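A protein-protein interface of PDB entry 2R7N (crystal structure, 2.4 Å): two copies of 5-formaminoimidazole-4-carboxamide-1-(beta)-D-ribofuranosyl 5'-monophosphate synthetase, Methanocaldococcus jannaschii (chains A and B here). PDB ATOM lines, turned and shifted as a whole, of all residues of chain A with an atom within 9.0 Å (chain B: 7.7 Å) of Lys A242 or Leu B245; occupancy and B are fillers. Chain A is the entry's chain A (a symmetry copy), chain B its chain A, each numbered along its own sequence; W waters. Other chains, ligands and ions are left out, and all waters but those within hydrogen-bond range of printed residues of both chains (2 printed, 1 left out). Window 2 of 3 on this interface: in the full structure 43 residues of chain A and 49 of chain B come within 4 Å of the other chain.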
ATOM      1  N   ILE A 239      15.510   4.842 -22.070  1.00  0.00           N
ATOM      2  CA  ILE A 239      16.000   6.122 -22.577  1.00  0.00           C
ATOM      3  C   ILE A 239      17.523   6.121 -22.475  1.00  0.00           C
ATOM      4  O   ILE A 239      18.071   5.717 -21.451  1.00  0.00           O
ATOM      5  CB  ILE A 239      15.449   7.274 -21.748  1.00  0.00           C
ATOM      6  CG1 ILE A 239      13.924   7.228 -21.741  1.00  0.00           C
ATOM      7  CG2 ILE A 239      15.957   8.618 -22.276  1.00  0.00           C
ATOM      8  CD1 ILE A 239      13.299   8.205 -20.789  1.00  0.00           C
ATOM      9  N   PRO A 240      18.211   6.514 -23.562  1.00  0.00           N
ATOM     10  CA  PRO A 240      19.670   6.666 -23.561  1.00  0.00           C
ATOM     11  C   PRO A 240      20.166   7.561 -22.425  1.00  0.00           C
ATOM     12  O   PRO A 240      19.520   8.555 -22.072  1.00  0.00           O
ATOM     13  CB  PRO A 240      19.952   7.332 -24.903  1.00  0.00           C
ATOM     14  CG  PRO A 240      18.805   6.913 -25.783  1.00  0.00           C
ATOM     15  CD  PRO A 240      17.618   6.803 -24.880  1.00  0.00           C
ATOM     16  N   ALA A 241      21.313   7.199 -21.865  1.00  0.00           N
ATOM     17  CA  ALA A 241      21.896   7.922 -20.740  1.00  0.00           C
ATOM     18  C   ALA A 241      21.994   9.432 -20.990  1.00  0.00           C
ATOM     19  O   ALA A 241      21.585  10.241 -20.140  1.00  0.00           O
ATOM     20  CB  ALA A 241      23.255   7.333 -20.389  1.00  0.00           C
ATOM     21  N   LYS A 242      22.516   9.811 -22.156  1.00  0.00           N
ATOM     22  CA  LYS A 242      22.637  11.227 -22.513  1.00  0.00           C
ATOM     23  C   LYS A 242      21.313  11.936 -22.331  1.00  0.00           C
ATOM     24  O   LYS A 242      21.231  12.966 -21.660  1.00  0.00           O
ATOM     25  CB  LYS A 242      23.117  11.391 -23.951  1.00  0.00           C
ATOM     26  CG  LYS A 242      24.598  11.090 -24.136  1.00  0.00           C
ATOM     27  CD  LYS A 242      25.006  11.152 -25.597  1.00  0.00           C
ATOM     28  CE  LYS A 242      26.390  10.550 -25.814  1.00  0.00           C
ATOM     29  NZ  LYS A 242      27.454  11.281 -25.071  1.00  0.00           N
ATOM     30  N   ASP A 243      20.269  11.369 -22.914  1.00  0.00           N
ATOM     31  CA  ASP A 243      18.922  11.923 -22.797  1.00  0.00           C
ATOM     32  C   ASP A 243      18.330  11.847 -21.391  1.00  0.00           C
ATOM     33  O   ASP A 243      17.604  12.740 -20.990  1.00  0.00           O
ATOM     34  CB  ASP A 243      18.019  11.252 -23.816  1.00  0.00           C
ATOM     35  CG  ASP A 243      18.465  11.520 -25.224  1.00  0.00           C
ATOM     36  OD1 ASP A 243      18.381  12.701 -25.639  1.00  0.00           O
ATOM     37  OD2 ASP A 243      18.917  10.570 -25.905  1.00  0.00           O
ATOM     38  N   GLN A 244      18.625  10.783 -20.638  1.00  0.00           N
ATOM     39  CA  GLN A 244      18.140  10.699 -19.260  1.00  0.00           C
ATOM     40  C   GLN A 244      18.678  11.872 -18.430  1.00  0.00           C
ATOM     41  O   GLN A 244      17.959  12.457 -17.626  1.00  0.00           O
ATOM     42  CB  GLN A 244      18.579   9.387 -18.601  1.00  0.00           C
ATOM     43  CG  GLN A 244      17.711   8.165 -18.869  1.00  0.00           C
ATOM     44  CD  GLN A 244      18.199   6.965 -18.093  1.00  0.00           C
ATOM     45  OE1 GLN A 244      18.299   7.014 -16.863  1.00  0.00           O
ATOM     46  NE2 GLN A 244      18.537   5.880 -18.803  1.00  0.00           N
ATOM     47  N   LEU A 245      19.960  12.189 -18.612  1.00  0.00           N
ATOM     48  CA  LEU A 245      20.606  13.293 -17.896  1.00  0.00           C
ATOM     49  C   LEU A 245      19.982  14.646 -18.218  1.00  0.00           C
ATOM     50  O   LEU A 245      19.938  15.531 -17.364  1.00  0.00           O
ATOM     51  CB  LEU A 245      22.108  13.339 -18.188  1.00  0.00           C
ATOM     52  CG  LEU A 245      22.891  12.079 -17.823  1.00  0.00           C
ATOM     53  CD1 LEU A 245      24.383  12.326 -17.979  1.00  0.00           C
ATOM     54  CD2 LEU A 245      22.560  11.624 -16.414  1.00  0.00           C
ATOM     55  N   GLU A 246      19.507  14.809 -19.446  1.00  0.00           N
ATOM     56  CA  GLU A 246      18.772  16.014 -19.808  1.00  0.00           C
ATOM     57  C   GLU A 246      17.348  16.030 -19.287  1.00  0.00           C
ATOM     58  O   GLU A 246      16.608  16.981 -19.539  1.00  0.00           O
ATOM     59  CB  GLU A 246      18.747  16.195 -21.314  1.00  0.00           C
ATOM     60  CG  GLU A 246      20.018  16.809 -21.831  1.00  0.00           C
ATOM     61  CD  GLU A 246      20.184  16.596 -23.300  1.00  0.00           C
ATOM     62  OE1 GLU A 246      20.034  15.436 -23.747  1.00  0.00           O
ATOM     63  OE2 GLU A 246      20.465  17.586 -24.007  1.00  0.00           O
ATOM     64  N   MET A 247      16.953  14.981 -18.571  1.00  0.00           N
ATOM     65  CA  MET A 247      15.592  14.925 -18.052  1.00  0.00           C
ATOM     66  C   MET A 247      15.556  15.144 -16.551  1.00  0.00           C
ATOM     67  O   MET A 247      16.515  14.840 -15.836  1.00  0.00           O
ATOM     68  CB  MET A 247      14.928  13.587 -18.380  1.00  0.00           C
ATOM     69  CG  MET A 247      14.897  13.222 -19.855  1.00  0.00           C
ATOM     70  SD  MET A 247      14.392  11.499 -20.072  1.00  0.00           S
ATOM     71  CE  MET A 247      12.651  11.604 -19.660  1.00  0.00           C
ATOM     72  N   ILE B 168      15.440  11.772 -29.746  1.00  0.00           N
ATOM     73  CA  ILE B 168      14.797  12.275 -28.533  1.00  0.00           C
ATOM     74  C   ILE B 168      15.288  13.695 -28.242  1.00  0.00           C
ATOM     75  O   ILE B 168      16.465  14.015 -28.449  1.00  0.00           O
ATOM     76  CB  ILE B 168      15.154  11.383 -27.325  1.00  0.00           C
ATOM     77  CG1 ILE B 168      14.621   9.957 -27.524  1.00  0.00           C
ATOM     78  CG2 ILE B 168      14.656  11.997 -26.011  1.00  0.00           C
ATOM     79  CD1 ILE B 168      15.081   8.978 -26.449  1.00  0.00           C
ATOM     80  N   SER B 170      14.708  17.239 -25.471  1.00  0.00           N
ATOM     81  CA  SER B 170      14.098  17.844 -24.293  1.00  0.00           C
ATOM     82  C   SER B 170      13.993  19.370 -24.400  1.00  0.00           C
ATOM     83  O   SER B 170      13.589  20.043 -23.439  1.00  0.00           O
ATOM     84  CB  SER B 170      14.840  17.433 -23.018  1.00  0.00           C
ATOM     85  OG  SER B 170      14.516  16.099 -22.643  1.00  0.00           O
ATOM     86  N   GLU B 174      17.842  21.405 -28.415  1.00  0.00           N
ATOM     87  CA  GLU B 174      18.257  20.020 -28.616  1.00  0.00           C
ATOM     88  C   GLU B 174      17.709  19.458 -29.926  1.00  0.00           C
ATOM     89  O   GLU B 174      18.408  18.743 -30.644  1.00  0.00           O
ATOM     90  CB  GLU B 174      17.850  19.142 -27.438  1.00  0.00           C
ATOM     91  CG  GLU B 174      18.252  17.690 -27.608  1.00  0.00           C
ATOM     92  CD  GLU B 174      18.380  16.958 -26.289  1.00  0.00           C
ATOM     93  OE1 GLU B 174      17.586  17.236 -25.358  1.00  0.00           O
ATOM     94  OE2 GLU B 174      19.283  16.100 -26.190  1.00  0.00           O
ATOM     95  N   LYS B 178      20.221  17.991 -32.782  1.00  0.00           N
ATOM     96  CA  LYS B 178      20.113  16.604 -33.228  1.00  0.00           C
ATOM     97  C   LYS B 178      19.657  16.463 -34.675  1.00  0.00           C
ATOM     98  O   LYS B 178      20.176  15.631 -35.426  1.00  0.00           O
ATOM     99  CB  LYS B 178      19.191  15.815 -32.298  1.00  0.00           C
ATOM    100  CG  LYS B 178      19.927  15.188 -31.136  1.00  0.00           C
ATOM    101  CD  LYS B 178      18.970  14.685 -30.096  1.00  0.00           C
ATOM    102  CE  LYS B 178      19.689  13.844 -29.076  1.00  0.00           C
ATOM    103  NZ  LYS B 178      18.737  13.337 -28.074  1.00  0.00           N
ATOM    104  N   LEU B 236      21.585  -0.366 -27.132  1.00  0.00           N
ATOM    105  CA  LEU B 236      22.215   0.852 -26.637  1.00  0.00           C
ATOM    106  C   LEU B 236      22.053   0.950 -25.117  1.00  0.00           C
ATOM    107  O   LEU B 236      23.027   1.127 -24.385  1.00  0.00           O
ATOM    108  CB  LEU B 236      21.629   2.089 -27.337  1.00  0.00           C
ATOM    109  CG  LEU B 236      21.965   3.497 -26.819  1.00  0.00           C
ATOM    110  CD1 LEU B 236      23.450   3.638 -26.556  1.00  0.00           C
ATOM    111  CD2 LEU B 236      21.509   4.553 -27.819  1.00  0.00           C
ATOM    112  N   ILE B 239      24.121  -0.850 -22.602  1.00  0.00           N
ATOM    113  CA  ILE B 239      25.441  -0.301 -22.295  1.00  0.00           C
ATOM    114  C   ILE B 239      25.313   0.569 -21.046  1.00  0.00           C
ATOM    115  O   ILE B 239      24.376   1.359 -20.940  1.00  0.00           O
ATOM    116  CB  ILE B 239      25.946   0.558 -23.446  1.00  0.00           C
ATOM    117  CG1 ILE B 239      25.973  -0.261 -24.732  1.00  0.00           C
ATOM    118  CG2 ILE B 239      27.328   1.134 -23.130  1.00  0.00           C
ATOM    119  CD1 ILE B 239      26.268   0.555 -25.957  1.00  0.00           C
ATOM    120  N   PRO B 240      26.219   0.380 -20.071  1.00  0.00           N
ATOM    121  CA  PRO B 240      26.277   1.222 -18.872  1.00  0.00           C
ATOM    122  C   PRO B 240      26.351   2.713 -19.205  1.00  0.00           C
ATOM    123  O   PRO B 240      27.000   3.114 -20.178  1.00  0.00           O
ATOM    124  CB  PRO B 240      27.572   0.780 -18.198  1.00  0.00           C
ATOM    125  CG  PRO B 240      27.776  -0.638 -18.661  1.00  0.00           C
ATOM    126  CD  PRO B 240      27.229  -0.694 -20.051  1.00  0.00           C
ATOM    127  N   ALA B 241      25.684   3.519 -18.389  1.00  0.00           N
ATOM    128  CA  ALA B 241      25.618   4.961 -18.598  1.00  0.00           C
ATOM    129  C   ALA B 241      26.999   5.597 -18.801  1.00  0.00           C
ATOM    130  O   ALA B 241      27.204   6.372 -19.751  1.00  0.00           O
ATOM    131  CB  ALA B 241      24.873   5.621 -17.447  1.00  0.00           C
ATOM    132  N   LYS B 242      27.946   5.258 -17.928  1.00  0.00           N
ATOM    133  CA  LYS B 242      29.309   5.785 -18.038  1.00  0.00           C
ATOM    134  C   LYS B 242      29.850   5.571 -19.435  1.00  0.00           C
ATOM    135  O   LYS B 242      30.323   6.504 -20.083  1.00  0.00           O
ATOM    136  CB  LYS B 242      30.235   5.129 -17.019  1.00  0.00           C
ATOM    137  CG  LYS B 242      30.024   5.630 -15.596  1.00  0.00           C
ATOM    138  CD  LYS B 242      30.881   4.870 -14.601  1.00  0.00           C
ATOM    139  CE  LYS B 242      30.446   5.146 -13.166  1.00  0.00           C
ATOM    140  NZ  LYS B 242      30.580   6.582 -12.793  1.00  0.00           N
ATOM    141  N   ASP B 243      29.760   4.336 -19.905  1.00  0.00           N
ATOM    142  CA  ASP B 243      30.211   3.987 -21.250  1.00  0.00           C
ATOM    143  C   ASP B 243      29.381   4.607 -22.374  1.00  0.00           C
ATOM    144  O   ASP B 243      29.923   4.948 -23.410  1.00  0.00           O
ATOM    145  CB  ASP B 243      30.275   2.476 -21.376  1.00  0.00           C
ATOM    146  CG  ASP B 243      31.271   1.876 -20.427  1.00  0.00           C
ATOM    147  OD1 ASP B 243      32.482   2.137 -20.623  1.00  0.00           O
ATOM    148  OD2 ASP B 243      30.852   1.169 -19.481  1.00  0.00           O
ATOM    149  N   GLN B 244      28.066   4.746 -22.184  1.00  0.00           N
ATOM    150  CA  GLN B 244      27.240   5.398 -23.201  1.00  0.00           C
ATOM    151  C   GLN B 244      27.713   6.839 -23.433  1.00  0.00           C
ATOM    152  O   GLN B 244      27.773   7.307 -24.565  1.00  0.00           O
ATOM    153  CB  GLN B 244      25.767   5.425 -22.780  1.00  0.00           C
ATOM    154  CG  GLN B 244      24.951   4.172 -23.072  1.00  0.00           C
ATOM    155  CD  GLN B 244      23.501   4.363 -22.691  1.00  0.00           C
ATOM    156  OE1 GLN B 244      22.842   5.286 -23.179  1.00  0.00           O
ATOM    157  NE2 GLN B 244      22.994   3.507 -21.793  1.00  0.00           N
ATOM    158  N   LEU B 245      28.019   7.546 -22.345  1.00  0.00           N
ATOM    159  CA  LEU B 245      28.496   8.930 -22.415  1.00  0.00           C
ATOM    160  C   LEU B 245      29.820   9.059 -23.158  1.00  0.00           C
ATOM    161  O   LEU B 245      30.069  10.066 -23.819  1.00  0.00           O
ATOM    162  CB  LEU B 245      28.630   9.541 -21.018  1.00  0.00           C
ATOM    163  CG  LEU B 245      27.350   9.572 -20.184  1.00  0.00           C
ATOM    164  CD1 LEU B 245      27.574  10.372 -18.911  1.00  0.00           C
ATOM    165  CD2 LEU B 245      26.194  10.140 -20.986  1.00  0.00           C
ATOM    166  N   GLU B 246      30.670   8.046 -23.045  1.00  0.00           N
ATOM    167  CA  GLU B 246      31.900   8.014 -23.826  1.00  0.00           C
ATOM    168  C   GLU B 246      31.684   7.633 -25.277  1.00  0.00           C
ATOM    169  O   GLU B 246      32.644   7.547 -26.043  1.00  0.00           O
ATOM    170  CB  GLU B 246      32.901   7.055 -23.208  1.00  0.00           C
ATOM    171  CG  GLU B 246      33.641   7.674 -22.056  1.00  0.00           C
ATOM    172  CD  GLU B 246      34.288   6.644 -21.189  1.00  0.00           C
ATOM    173  OE1 GLU B 246      33.591   5.677 -20.806  1.00  0.00           O
ATOM    174  OE2 GLU B 246      35.490   6.800 -20.891  1.00  0.00           O
ATOM    175  N   MET B 247      30.433   7.393 -25.661  1.00  0.00           N
ATOM    176  CA  MET B 247      30.155   7.007 -27.038  1.00  0.00           C
ATOM    177  C   MET B 247      29.490   8.130 -27.810  1.00  0.00           C
ATOM    178  O   MET B 247      28.791   8.974 -27.241  1.00  0.00           O
ATOM    179  CB  MET B 247      29.268   5.763 -27.097  1.00  0.00           C
ATOM    180  CG  MET B 247      29.802   4.549 -26.355  1.00  0.00           C
ATOM    181  SD  MET B 247      28.528   3.272 -26.229  1.00  0.00           S
ATOM    182  CE  MET B 247      28.461   2.694 -27.923  1.00  0.00           C
ATOM    183  N   ASN B 248      29.711   8.133 -29.117  1.00  0.00           N
ATOM    184  CA  ASN B 248      28.973   9.022 -29.994  1.00  0.00           C
ATOM    185  C   ASN B 248      28.048   8.166 -30.841  1.00  0.00           C
ATOM    186  O   ASN B 248      28.402   7.735 -31.939  1.00  0.00           O
ATOM    187  CB  ASN B 248      29.918   9.867 -30.853  1.00  0.00           C
ATOM    188  CG  ASN B 248      30.682  10.901 -30.032  1.00  0.00           C
ATOM    189  OD1 ASN B 248      30.126  11.513 -29.116  1.00  0.00           O
ATOM    190  ND2 ASN B 248      31.959  11.096 -30.357  1.00  0.00           N
ATOM    191  N   ILE B 249      26.864   7.907 -30.301  1.00  0.00           N
ATOM    192  CA  ILE B 249      25.951   6.954 -30.902  1.00  0.00           C
ATOM    193  C   ILE B 249      24.530   7.484 -30.841  1.00  0.00           C
ATOM    194  O   ILE B 249      24.114   8.060 -29.841  1.00  0.00           O
ATOM    195  CB  ILE B 249      26.039   5.580 -30.194  1.00  0.00           C
ATOM    196  CG1 ILE B 249      25.270   4.507 -30.972  1.00  0.00           C
ATOM    197  CG2 ILE B 249      25.550   5.682 -28.753  1.00  0.00           C
ATOM    198  CD1 ILE B 249      25.524   3.100 -30.473  1.00  0.00           C
ATOM    199  N   ASN B 250      23.792   7.306 -31.926  1.00  0.00           N
ATOM    200  CA  ASN B 250      22.402   7.709 -31.946  1.00  0.00           C
ATOM    201  C   ASN B 250      21.477   6.513 -31.792  1.00  0.00           C
ATOM    202  O   ASN B 250      21.684   5.470 -32.419  1.00  0.00           O
ATOM    203  CB  ASN B 250      22.086   8.472 -33.232  1.00  0.00           C
ATOM    204  CG  ASN B 250      22.962   9.701 -33.408  1.00  0.00           C
ATOM    205  OD1 ASN B 250      23.641   9.850 -34.424  1.00  0.00           O
ATOM    206  ND2 ASN B 250      22.965  10.581 -32.406  1.00  0.00           N
ATOM    207  N   PRO B 251      20.460   6.653 -30.939  1.00  0.00           N
ATOM    208  CA  PRO B 251      19.436   5.623 -30.838  1.00  0.00           C
ATOM    209  C   PRO B 251      18.751   5.398 -32.175  1.00  0.00           C
ATOM    210  O   PRO B 251      18.423   6.354 -32.874  1.00  0.00           O
ATOM    211  CB  PRO B 251      18.433   6.204 -29.831  1.00  0.00           C
ATOM    212  CG  PRO B 251      18.746   7.664 -29.745  1.00  0.00           C
ATOM    213  CD  PRO B 251      20.219   7.774 -30.017  1.00  0.00           C
HETATM  214  O   HOH W   1      16.670  14.376 -23.805  1.00  0.00           O
HETATM  215  O   HOH W   2      23.320   7.895 -24.537  1.00  0.00           O
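OE1 of Glu A246 lies close to OE2 of Glu B174, at 2.6 Å. The side-chain amino group of Lys A242 sits at hydrogen-bond distance from the backbone carbonyl oxygen of Leu B245 (3.1 Å). O of Met B247 lies close to NZ of Lys A242. The backbone NH of Ala A241 lies within hydrogen-bond range of the side-chain amide oxygen of Gln B244 (2.8 Å). The side-chain amino group (NZ) of Lys B178 is in salt-bridge range of the side-chain carboxylate (OD1) of Asp A243 (2.5 Å).
The side-chain carboxylate of Glu B174 is in salt-bridge range of the side-chain amino group of Lys B178, 3.4 Å away. The backbone NH (N) of Ser B170 is in hydrogen-bond range of the side-chain carboxylate (OE1) of Glu B174 (2.9 Å). O of Ile B168 lies within hydrogen-bond range of NZ of Lys B178, 2.4 Å away. The side-chain amide nitrogen (NE2) of Gln B244 is in hydrogen-bond range of the backbone carbonyl oxygen (O) of Ile B239 (2.7 Å).
Among the printed residues, pairs that only touch across the chains: Pro A240 with Gln B244 (3.5 Å), Asp A243 with Glu B174 (3.6 Å), Asp A243 with Ile B168 (3.6 Å), Pro A240 with Ile B168 (3.7 Å), Lys A242 with Gln B244 (3.7 Å), Ala A241 with Ala B241 (3.8 Å), Glu A246 with Ser B170 (3.8 Å) and Leu A245 with Leu B245 (3.9 Å).
Leu B245 touches two residues of chain A. Of chain B, only Ala B241 (3.8 Å) and Gln B244 (2.8 Å) come within 4 Å of Ala A241. Of the printed residues of chain B, Glu A246 touches Ser B170 (3.8 Å) and Glu B174 (2.6 Å). Of the printed residues of chain B, Pro A240 touches Ile B168 (3.7 Å) and Gln B244 (3.5 Å). Of the printed residues of chain B, Leu A245 touches Leu B245 (3.9 Å). Of the printed residues of chain B, Asp A243 touches Ile B168, Glu B174 and Lys B178. Printed residues of chain A within 4 Å of Ile B168: Pro A240 and Asp A243. Ile B249 touches none of the printed residues of chain A. The nearest residue of chain A that does not touch Leu B245 is Ala A241 (4.1 Å).
Hydrophobic or aromatic side chains of chain A that line the printed part of chain B: Pro A240, Ala A241 and Leu A245. Of the 18 printed residues of chain B, 8 touch a printed residue of chain A. Hydrophobic or aromatic side chains of chain B within 4 Å of the printed part of chain A: Ile B168, Ala B241 and Leu B245. Among the printed residues, 13 pairs touch across the chains. Among the printed residues, Asp or Glu carboxylates within 4 Å of a Lys or Arg side-chain nitrogen of the other chain: Asp A243 with Lys B178.
Ala A241 touches its own counterpart, Ala B241. Lys A242 touches Gln B244, but with the chains exchanged Gln A244 does not touch Lys B242 (9.5 Å). Lys A242 touches Leu B245, but with the chains exchanged Leu A245 does not touch Lys B242 (7.9 Å). Lys A242 touches Met B247, but with the chains exchanged Met A247 does not touch Lys B242 (14.7 Å). Of the 13 pairs that touch across the chains among the printed residues, 2 have their exchanged pair printed and touching as well.
Water W2 lies within hydrogen-bond range of OE1 of Gln B244 (3.0 Å), N of Lys A242 (3.2 Å) and N of Ala A241 (3.4 Å). Water W1 lies within hydrogen-bond range of the side-chain hydroxyl (OG) of Ser B170 (3.0 Å), the side-chain carboxylate (OD1) of Asp A243 (3.0 Å) and the side-chain carboxylate (OE1) of Glu B174 (3.4 Å).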
